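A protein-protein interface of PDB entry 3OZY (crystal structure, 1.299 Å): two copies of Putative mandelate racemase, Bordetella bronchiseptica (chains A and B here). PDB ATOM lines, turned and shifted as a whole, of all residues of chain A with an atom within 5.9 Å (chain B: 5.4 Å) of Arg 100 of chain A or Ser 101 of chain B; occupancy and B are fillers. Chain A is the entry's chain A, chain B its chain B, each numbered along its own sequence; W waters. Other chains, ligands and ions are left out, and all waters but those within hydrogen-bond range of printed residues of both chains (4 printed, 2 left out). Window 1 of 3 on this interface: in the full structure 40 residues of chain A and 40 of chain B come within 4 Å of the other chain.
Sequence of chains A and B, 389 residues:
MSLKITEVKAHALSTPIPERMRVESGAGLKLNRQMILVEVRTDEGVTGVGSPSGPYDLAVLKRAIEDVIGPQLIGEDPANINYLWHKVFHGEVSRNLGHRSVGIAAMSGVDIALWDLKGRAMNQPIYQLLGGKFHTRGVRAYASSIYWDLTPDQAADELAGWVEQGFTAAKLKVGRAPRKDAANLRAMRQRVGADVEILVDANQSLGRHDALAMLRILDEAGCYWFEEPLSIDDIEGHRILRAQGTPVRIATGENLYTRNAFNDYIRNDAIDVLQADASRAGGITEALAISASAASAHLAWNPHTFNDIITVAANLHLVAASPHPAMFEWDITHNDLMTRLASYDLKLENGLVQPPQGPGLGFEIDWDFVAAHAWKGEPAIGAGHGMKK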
ATOM      1  N   LEU A  97     -12.263   8.666   0.124  1.00  0.00           N
ATOM      2  CA  LEU A  97     -12.771   9.883  -0.513  1.00  0.00           C
ATOM      3  C   LEU A  97     -12.814  11.073   0.440  1.00  0.00           C
ATOM      4  O   LEU A  97     -13.064  12.194   0.002  1.00  0.00           O
ATOM      5  CB  LEU A  97     -14.146   9.661  -1.156  1.00  0.00           C
ATOM      6  CG  LEU A  97     -14.133   8.763  -2.397  1.00  0.00           C
ATOM      7  CD1 LEU A  97     -15.554   8.434  -2.851  1.00  0.00           C
ATOM      8  CD2 LEU A  97     -13.330   9.389  -3.535  1.00  0.00           C
ATOM      9  N   GLY A  98     -12.536  10.838   1.726  1.00  0.00           N
ATOM     10  CA  GLY A  98     -12.529  11.885   2.740  1.00  0.00           C
ATOM     11  C   GLY A  98     -13.817  11.928   3.533  1.00  0.00           C
ATOM     12  O   GLY A  98     -14.905  11.746   2.985  1.00  0.00           O
ATOM     13  N   HIS A  99     -13.703  12.171   4.833  1.00  0.00           N
ATOM     14  CA  HIS A  99     -14.857  12.021   5.708  1.00  0.00           C
ATOM     15  C   HIS A  99     -15.959  13.091   5.540  1.00  0.00           C
ATOM     16  O   HIS A  99     -17.092  12.836   5.938  1.00  0.00           O
ATOM     17  CB  HIS A  99     -14.418  11.889   7.175  1.00  0.00           C
ATOM     18  CG  HIS A  99     -13.825  13.133   7.767  1.00  0.00           C
ATOM     19  ND1 HIS A  99     -14.070  13.516   9.069  1.00  0.00           N
ATOM     20  CD2 HIS A  99     -12.995  14.071   7.251  1.00  0.00           C
ATOM     21  CE1 HIS A  99     -13.419  14.637   9.328  1.00  0.00           C
ATOM     22  NE2 HIS A  99     -12.761  14.998   8.240  1.00  0.00           N
ATOM     23  N   ARG A 100     -15.638  14.256   4.961  1.00  0.00           N
ATOM     24  CA  ARG A 100     -16.643  15.314   4.730  1.00  0.00           C
ATOM     25  C   ARG A 100     -16.506  15.792   3.291  1.00  0.00           C
ATOM     26  O   ARG A 100     -15.897  16.829   3.014  1.00  0.00           O
ATOM     27  CB  ARG A 100     -16.474  16.470   5.725  1.00  0.00           C
ATOM     28  CG  ARG A 100     -16.258  16.030   7.189  1.00  0.00           C
ATOM     29  CD  ARG A 100     -17.522  15.419   7.829  1.00  0.00           C
ATOM     30  NE  ARG A 100     -17.208  14.936   9.179  1.00  0.00           N
ATOM     31  CZ  ARG A 100     -17.086  15.712  10.250  1.00  0.00           C
ATOM     32  NH1 ARG A 100     -17.307  17.014  10.156  1.00  0.00           N
ATOM     33  NH2 ARG A 100     -16.755  15.180  11.428  1.00  0.00           N
ATOM     34  N   SER A 101     -17.080  15.026   2.371  1.00  0.00           N
ATOM     35  CA  SER A 101     -16.629  15.094   0.994  1.00  0.00           C
ATOM     36  C   SER A 101     -17.723  14.842  -0.025  1.00  0.00           C
ATOM     37  O   SER A 101     -18.825  14.393   0.299  1.00  0.00           O
ATOM     38  CB  SER A 101     -15.564  14.016   0.783  1.00  0.00           C
ATOM     39  OG  SER A 101     -16.176  12.728   0.815  1.00  0.00           O
ATOM     40  N   VAL A 102     -17.371  15.097  -1.282  1.00  0.00           N
ATOM     41  CA  VAL A 102     -18.172  14.674  -2.422  1.00  0.00           C
ATOM     42  C   VAL A 102     -18.490  13.167  -2.379  1.00  0.00           C
ATOM     43  O   VAL A 102     -19.506  12.735  -2.926  1.00  0.00           O
ATOM     44  CB  VAL A 102     -17.473  15.065  -3.753  1.00  0.00           C
ATOM     45  CG1 VAL A 102     -16.128  14.357  -3.899  1.00  0.00           C
ATOM     46  CG2 VAL A 102     -18.375  14.813  -4.948  1.00  0.00           C
ATOM     47  N   ILE A 104     -19.328  11.564   0.309  1.00  0.00           N
ATOM     48  CA  ILE A 104     -20.512  11.484   1.162  1.00  0.00           C
ATOM     49  C   ILE A 104     -21.776  11.870   0.377  1.00  0.00           C
ATOM     50  O   ILE A 104     -22.823  11.239   0.537  1.00  0.00           O
ATOM     51  CB  ILE A 104     -20.354  12.358   2.436  1.00  0.00           C
ATOM     52  CG1 ILE A 104     -19.085  11.966   3.222  1.00  0.00           C
ATOM     53  CG2 ILE A 104     -21.608  12.272   3.305  1.00  0.00           C
ATOM     54  CD1 ILE A 104     -19.159  10.580   3.897  1.00  0.00           C
ATOM     55  N   LEU A 256     -21.972  20.853   5.302  1.00  0.00           N
ATOM     56  CA  LEU A 256     -21.494  20.020   6.406  1.00  0.00           C
ATOM     57  C   LEU A 256     -21.982  18.604   6.173  1.00  0.00           C
ATOM     58  O   LEU A 256     -23.076  18.395   5.657  1.00  0.00           O
ATOM     59  CB  LEU A 256     -22.038  20.539   7.735  1.00  0.00           C
ATOM     60  CG  LEU A 256     -21.551  21.922   8.141  1.00  0.00           C
ATOM     61  CD1 LEU A 256     -22.358  22.393   9.340  1.00  0.00           C
ATOM     62  CD2 LEU A 256     -20.068  21.881   8.465  1.00  0.00           C
ATOM     63  N   TYR A 257     -21.165  17.627   6.550  1.00  0.00           N
ATOM     64  CA  TYR A 257     -21.406  16.238   6.180  1.00  0.00           C
ATOM     65  C   TYR A 257     -21.459  15.304   7.379  1.00  0.00           C
ATOM     66  O   TYR A 257     -20.585  15.351   8.252  1.00  0.00           O
ATOM     67  CB  TYR A 257     -20.312  15.767   5.216  1.00  0.00           C
ATOM     68  CG  TYR A 257     -20.356  16.496   3.893  1.00  0.00           C
ATOM     69  CD1 TYR A 257     -21.100  15.992   2.827  1.00  0.00           C
ATOM     70  CD2 TYR A 257     -19.663  17.692   3.701  1.00  0.00           C
ATOM     71  CE1 TYR A 257     -21.158  16.659   1.619  1.00  0.00           C
ATOM     72  CE2 TYR A 257     -19.723  18.372   2.488  1.00  0.00           C
ATOM     73  CZ  TYR A 257     -20.470  17.844   1.451  1.00  0.00           C
ATOM     74  OH  TYR A 257     -20.555  18.486   0.230  1.00  0.00           O
ATOM     75  N   THR A 258     -22.464  14.427   7.373  1.00  0.00           N
ATOM     76  CA  THR A 258     -22.722  13.416   8.410  1.00  0.00           C
ATOM     77  C   THR A 258     -23.171  14.026   9.726  1.00  0.00           C
ATOM     78  O   THR A 258     -22.999  15.222   9.986  1.00  0.00           O
ATOM     79  CB  THR A 258     -21.524  12.455   8.698  1.00  0.00           C
ATOM     80  OG1 THR A 258     -20.599  13.080   9.601  1.00  0.00           O
ATOM     81  CG2 THR A 258     -20.833  12.000   7.412  1.00  0.00           C
ATOM     82  N   ASN A 260     -21.749  13.711  12.378  1.00  0.00           N
ATOM     83  CA  ASN A 260     -20.577  14.129  13.148  1.00  0.00           C
ATOM     84  C   ASN A 260     -20.351  15.634  13.088  1.00  0.00           C
ATOM     85  O   ASN A 260     -19.971  16.259  14.080  1.00  0.00           O
ATOM     86  CB  ASN A 260     -19.332  13.401  12.647  1.00  0.00           C
ATOM     87  CG  ASN A 260     -19.498  11.908  12.666  1.00  0.00           C
ATOM     88  OD1 ASN A 260     -19.497  11.244  11.619  1.00  0.00           O
ATOM     89  ND2 ASN A 260     -19.661  11.364  13.854  1.00  0.00           N
ATOM     90  N   ALA A 261     -20.581  16.223  11.917  1.00  0.00           N
ATOM     91  CA  ALA A 261     -20.416  17.667  11.761  1.00  0.00           C
ATOM     92  C   ALA A 261     -21.406  18.407  12.650  1.00  0.00           C
ATOM     93  O   ALA A 261     -21.057  19.359  13.355  1.00  0.00           O
ATOM     94  CB  ALA A 261     -20.625  18.074  10.303  1.00  0.00           C
ATOM     95  N   ASP A 264     -20.688  18.340  16.363  1.00  0.00           N
ATOM     96  CA  ASP A 264     -19.687  19.332  16.748  1.00  0.00           C
ATOM     97  C   ASP A 264     -20.301  20.723  16.903  1.00  0.00           C
ATOM     98  O   ASP A 264     -19.946  21.454  17.817  1.00  0.00           O
ATOM     99  CB  ASP A 264     -18.530  19.368  15.753  1.00  0.00           C
ATOM    100  CG  ASP A 264     -17.566  18.223  15.941  1.00  0.00           C
ATOM    101  OD1 ASP A 264     -17.549  17.622  17.035  1.00  0.00           O
ATOM    102  OD2 ASP A 264     -16.819  17.932  14.995  1.00  0.00           O
ATOM    103  N   VAL B  93     -13.020  24.043  -4.644  1.00  0.00           N
ATOM    104  CA  VAL B  93     -12.846  22.782  -3.922  1.00  0.00           C
ATOM    105  C   VAL B  93     -13.700  22.643  -2.659  1.00  0.00           C
ATOM    106  O   VAL B  93     -14.365  21.622  -2.456  1.00  0.00           O
ATOM    107  CB  VAL B  93     -11.359  22.503  -3.637  1.00  0.00           C
ATOM    108  CG1 VAL B  93     -11.203  21.292  -2.720  1.00  0.00           C
ATOM    109  CG2 VAL B  93     -10.602  22.317  -4.956  1.00  0.00           C
ATOM    110  N   LEU B  97     -16.197  20.084  -4.005  1.00  0.00           N
ATOM    111  CA  LEU B  97     -15.670  18.753  -3.706  1.00  0.00           C
ATOM    112  C   LEU B  97     -15.787  18.393  -2.230  1.00  0.00           C
ATOM    113  O   LEU B  97     -15.562  17.238  -1.868  1.00  0.00           O
ATOM    114  CB  LEU B  97     -14.228  18.592  -4.196  1.00  0.00           C
ATOM    115  CG  LEU B  97     -14.102  18.573  -5.722  1.00  0.00           C
ATOM    116  CD1 LEU B  97     -12.640  18.661  -6.108  1.00  0.00           C
ATOM    117  CD2 LEU B  97     -14.751  17.337  -6.335  1.00  0.00           C
ATOM    118  N   GLY B  98     -16.170  19.354  -1.388  1.00  0.00           N
ATOM    119  CA  GLY B  98     -16.326  19.112   0.044  1.00  0.00           C
ATOM    120  C   GLY B  98     -15.134  19.623   0.834  1.00  0.00           C
ATOM    121  O   GLY B  98     -13.979  19.466   0.422  1.00  0.00           O
ATOM    122  N   HIS B  99     -15.397  20.204   1.994  1.00  0.00           N
ATOM    123  CA  HIS B  99     -14.339  20.897   2.726  1.00  0.00           C
ATOM    124  C   HIS B  99     -13.268  20.001   3.366  1.00  0.00           C
ATOM    125  O   HIS B  99     -12.188  20.491   3.674  1.00  0.00           O
ATOM    126  CB  HIS B  99     -14.939  21.874   3.746  1.00  0.00           C
ATOM    127  CG  HIS B  99     -15.637  21.214   4.900  1.00  0.00           C
ATOM    128  ND1 HIS B  99     -15.548  21.702   6.188  1.00  0.00           N
ATOM    129  CD2 HIS B  99     -16.449  20.131   4.963  1.00  0.00           C
ATOM    130  CE1 HIS B  99     -16.268  20.941   6.996  1.00  0.00           C
ATOM    131  NE2 HIS B  99     -16.822  19.978   6.280  1.00  0.00           N
ATOM    132  N   ARG B 100     -13.554  18.711   3.552  1.00  0.00           N
ATOM    133  CA  ARG B 100     -12.576  17.780   4.142  1.00  0.00           C
ATOM    134  C   ARG B 100     -12.565  16.513   3.300  1.00  0.00           C
ATOM    135  O   ARG B 100     -13.174  15.502   3.654  1.00  0.00           O
ATOM    136  CB  ARG B 100     -12.908  17.464   5.608  1.00  0.00           C
ATOM    137  CG  ARG B 100     -13.242  18.683   6.468  1.00  0.00           C
ATOM    138  CD  ARG B 100     -12.046  19.615   6.721  1.00  0.00           C
ATOM    139  NE  ARG B 100     -12.499  20.786   7.479  1.00  0.00           N
ATOM    140  CZ  ARG B 100     -12.732  20.792   8.791  1.00  0.00           C
ATOM    141  NH1 ARG B 100     -12.522  19.697   9.511  1.00  0.00           N
ATOM    142  NH2 ARG B 100     -13.191  21.898   9.380  1.00  0.00           N
ATOM    143  N   SER B 101     -11.870  16.581   2.169  1.00  0.00           N
ATOM    144  CA  SER B 101     -12.179  15.671   1.074  1.00  0.00           C
ATOM    145  C   SER B 101     -10.984  15.302   0.226  1.00  0.00           C
ATOM    146  O   SER B 101      -9.911  15.895   0.316  1.00  0.00           O
ATOM    147  CB  SER B 101     -13.189  16.338   0.135  1.00  0.00           C
ATOM    148  OG  SER B 101     -12.558  17.415  -0.560  1.00  0.00           O
ATOM    149  N   VAL B 102     -11.222  14.326  -0.648  1.00  0.00           N
ATOM    150  CA  VAL B 102     -10.297  13.998  -1.725  1.00  0.00           C
ATOM    151  C   VAL B 102      -9.933  15.235  -2.571  1.00  0.00           C
ATOM    152  O   VAL B 102      -8.854  15.299  -3.142  1.00  0.00           O
ATOM    153  CB  VAL B 102     -10.854  12.849  -2.599  1.00  0.00           C
ATOM    154  CG1 VAL B 102     -12.151  13.271  -3.293  1.00  0.00           C
ATOM    155  CG2 VAL B 102      -9.819  12.400  -3.617  1.00  0.00           C
ATOM    156  N   GLY B 103     -10.830  16.220  -2.635  1.00  0.00           N
ATOM    157  CA  GLY B 103     -10.507  17.480  -3.293  1.00  0.00           C
ATOM    158  C   GLY B 103      -9.387  18.250  -2.615  1.00  0.00           C
ATOM    159  O   GLY B 103      -8.575  18.894  -3.278  1.00  0.00           O
ATOM    160  N   ILE B 104      -9.352  18.192  -1.287  1.00  0.00           N
ATOM    161  CA  ILE B 104      -8.263  18.798  -0.534  1.00  0.00           C
ATOM    162  C   ILE B 104      -6.940  18.064  -0.801  1.00  0.00           C
ATOM    163  O   ILE B 104      -5.905  18.700  -0.956  1.00  0.00           O
ATOM    164  CB  ILE B 104      -8.584  18.844   0.979  1.00  0.00           C
ATOM    165  CG1 ILE B 104      -9.922  19.576   1.228  1.00  0.00           C
ATOM    166  CG2 ILE B 104      -7.436  19.492   1.758  1.00  0.00           C
ATOM    167  CD1 ILE B 104      -9.898  21.094   0.916  1.00  0.00           C
ATOM    168  N   ALA B 105      -6.982  16.734  -0.869  1.00  0.00           N
ATOM    169  CA  ALA B 105      -5.786  15.971  -1.229  1.00  0.00           C
ATOM    170  C   ALA B 105      -5.322  16.362  -2.643  1.00  0.00           C
ATOM    171  O   ALA B 105      -4.136  16.628  -2.869  1.00  0.00           O
ATOM    172  CB  ALA B 105      -6.043  14.470  -1.133  1.00  0.00           C
ATOM    173  N   ALA B 106      -6.266  16.423  -3.585  1.00  0.00           N
ATOM    174  CA  ALA B 106      -5.963  16.861  -4.948  1.00  0.00           C
ATOM    175  C   ALA B 106      -5.269  18.233  -4.965  1.00  0.00           C
ATOM    176  O   ALA B 106      -4.242  18.422  -5.637  1.00  0.00           O
ATOM    177  CB  ALA B 106      -7.240  16.889  -5.774  1.00  0.00           C
ATOM    178  N   ASP B 233     -13.748  11.238  13.610  1.00  0.00           N
ATOM    179  CA  ASP B 233     -14.964  12.019  13.819  1.00  0.00           C
ATOM    180  C   ASP B 233     -15.313  12.198  15.284  1.00  0.00           C
ATOM    181  O   ASP B 233     -16.202  12.985  15.607  1.00  0.00           O
ATOM    182  CB  ASP B 233     -16.136  11.381  13.075  1.00  0.00           C
ATOM    183  CG  ASP B 233     -16.006  11.524  11.574  1.00  0.00           C
ATOM    184  OD1 ASP B 233     -15.659  12.638  11.143  1.00  0.00           O
ATOM    185  OD2 ASP B 233     -16.250  10.542  10.839  1.00  0.00           O
ATOM    186  N   TYR B 257      -8.397  17.154   7.508  1.00  0.00           N
ATOM    187  CA  TYR B 257      -8.069  18.047   6.401  1.00  0.00           C
ATOM    188  C   TYR B 257      -8.096  19.514   6.803  1.00  0.00           C
ATOM    189  O   TYR B 257      -9.048  19.972   7.440  1.00  0.00           O
ATOM    190  CB  TYR B 257      -9.050  17.810   5.239  1.00  0.00           C
ATOM    191  CG  TYR B 257      -8.884  16.431   4.637  1.00  0.00           C
ATOM    192  CD1 TYR B 257      -8.031  16.221   3.553  1.00  0.00           C
ATOM    193  CD2 TYR B 257      -9.559  15.328   5.168  1.00  0.00           C
ATOM    194  CE1 TYR B 257      -7.851  14.958   3.013  1.00  0.00           C
ATOM    195  CE2 TYR B 257      -9.390  14.066   4.631  1.00  0.00           C
ATOM    196  CZ  TYR B 257      -8.537  13.888   3.554  1.00  0.00           C
ATOM    197  OH  TYR B 257      -8.355  12.622   3.023  1.00  0.00           O
ATOM    198  N   ARG B 280      -1.824  15.667   1.702  1.00  0.00           N
ATOM    199  CA  ARG B 280      -3.232  15.333   1.942  1.00  0.00           C
ATOM    200  C   ARG B 280      -4.040  16.494   2.505  1.00  0.00           C
ATOM    201  O   ARG B 280      -5.183  16.710   2.106  1.00  0.00           O
ATOM    202  CB  ARG B 280      -3.345  14.157   2.929  1.00  0.00           C
ATOM    203  CG  ARG B 280      -2.701  12.869   2.438  1.00  0.00           C
ATOM    204  CD  ARG B 280      -2.532  11.836   3.551  1.00  0.00           C
ATOM    205  NE  ARG B 280      -3.784  11.191   3.940  1.00  0.00           N
ATOM    206  CZ  ARG B 280      -4.290  10.132   3.320  1.00  0.00           C
ATOM    207  NH1 ARG B 280      -3.661   9.629   2.264  1.00  0.00           N
ATOM    208  NH2 ARG B 280      -5.418   9.575   3.745  1.00  0.00           N
HETATM  209  O   HOH W   1     -15.846  15.546  14.176  1.00  0.00           O
HETATM  210  O   HOH W   2     -16.465  15.225  17.459  1.00  0.00           O
HETATM  211  O   HOH W   3     -11.144  17.087   8.864  1.00  0.00           O
HETATM  212  O   HOH W   4     -18.593  18.628   7.868  1.00  0.00           O
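The backbone NH (N) of Val 102 of chain B sits at hydrogen-bond distance from the backbone carbonyl oxygen (O) of Leu 97 of chain A. ND1 of His 99 of chain A lies within hydrogen-bond range of OD1 of Asp 233 of chain B (2.8 Å). O of Arg 100 of chain A lies within hydrogen-bond range of N of Arg 100 of chain B, 3.1 Å away. The guanidinium group of Arg 100 of chain A lies within salt-bridge range of the side-chain carboxylate of Asp 233 of chain B, 2.8 Å away. The backbone carbonyl oxygen of Leu 97 of chain B sits at hydrogen-bond distance from the backbone NH of Val 102 of chain A. OD1 of Asn 260 of chain A lies close to OD2 of Asp 233 of chain B, at 3.4 Å.
The side-chain hydroxyl (OG) of Ser 101 of chain A sits close to the backbone carbonyl oxygen (O) of Leu 97 of chain A (3.3 Å). OG1 of Thr 258 of chain A sits at hydrogen-bond distance from OD1 of Asn 260 of chain A, 2.9 Å away. The backbone carbonyl oxygen of Val 93 of chain B lies within hydrogen-bond range of the backbone NH of Gly 98 of chain B. The side-chain hydroxyl (OG) of Ser 101 of chain B lies within hydrogen-bond range of the backbone carbonyl oxygen (O) of Gly 98 of chain B, 2.7 Å away. The side-chain hydroxyl (OG) of Ser 101 of chain B sits at hydrogen-bond distance from the backbone NH (N) of Gly 103 of chain B (3.0 Å). The backbone NH of Ile 104 of chain B lies within hydrogen-bond range of the side-chain hydroxyl of Ser 101 of chain B (3.4 Å).
O of Leu 97 of chain A touches CA of Ser 101 of chain B, at 3.7 Å. Gly 98 of chain A touches Arg 100 of chain B (C to O, 3.6 Å). His 99 of chain A touches Arg 100 of chain B (N to O, 3.6 Å). Gly 98 of chain B touches Arg 100 of chain A (C to O, 3.6 Å). Arg 100 of chain A touches His 99 of chain B. CB of Ser 101 of chain B touches O of Arg 100 of chain A (3.98 Å). Ser 101 of chain A touches Leu 97 of chain B. Ser 101 of chain A touches Ser 101 of chain B.
Printed residues of chain B within 4 Å of Arg 100 of chain A: Gly 98, His 99, Arg 100, Ser 101 and Asp 233. Of the printed residues of chain A, Ser 101 of chain B touches Leu 97, Arg 100 and Ser 101. Printed residues of chain B within 4 Å of Val 102 of chain A: Leu 97 (2.9 Å). Of the printed residues of chain B, Leu 97 of chain A touches Ser 101 and Val 102. Printed residues of chain B within 4 Å of Ser 101 of chain A: Leu 97 and Ser 101. Of the printed residues of chain B, His 99 of chain A touches Arg 100 and Asp 233. The nearest printed residue of chain A that does not touch Ser 101 of chain B is Gly 98 of chain A (4.2 Å). The nearest printed residue of chain A that does not touch Arg 100 of chain B is Ser 101 of chain A (4.02 Å).
Hydrophobic or aromatic side chains of chain B that line the printed part of chain A: His 99 and Val 102. Along chain A the printed residues that touch a printed residue of chain B span positions 97 to 260.
Leu 97 of chain A touches Val 102 of chain B, and with the chains exchanged Val 102 of chain A touches Leu 97 of chain B. Gly 98 of chain A touches Arg 100 of chain B, and with the chains exchanged Arg 100 of chain A touches Gly 98 of chain B. His 99 of chain A touches Arg 100 of chain B, and with the chains exchanged Arg 100 of chain A touches His 99 of chain B. Arg 100 of chain A touches its own counterpart, Arg 100 of chain B. Positions printed for both chains: 97, 98, 99, 100, 101, 102, 104 and 257.
Water W2 lies within hydrogen-bond range of the side-chain carboxylate of Asp 264 of chain A (2.7 Å) and the backbone carbonyl oxygen of Asp 233 of chain B (2.9 Å). Water W1 lies within hydrogen-bond range of the side-chain carboxylate of Asp 264 of chain A (2.7 Å), the guanidinium group of Arg 100 of chain A (2.9 Å) and the backbone carbonyl oxygen of Asp 233 of chain B (3.0 Å). Water W3 lies within hydrogen-bond range of NE2 of His 99 of chain A, NH1 of Arg 100 of chain B and N of Tyr 257 of chain B. Water W4 lies within hydrogen-bond range of a ring nitrogen (NE2) of His 99 of chain B (2.7 Å), the backbone NH (N) of Tyr 257 of chain A (3.1 Å) and the guanidinium group (NH1) of Arg 100 of chain A (3.1 Å).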
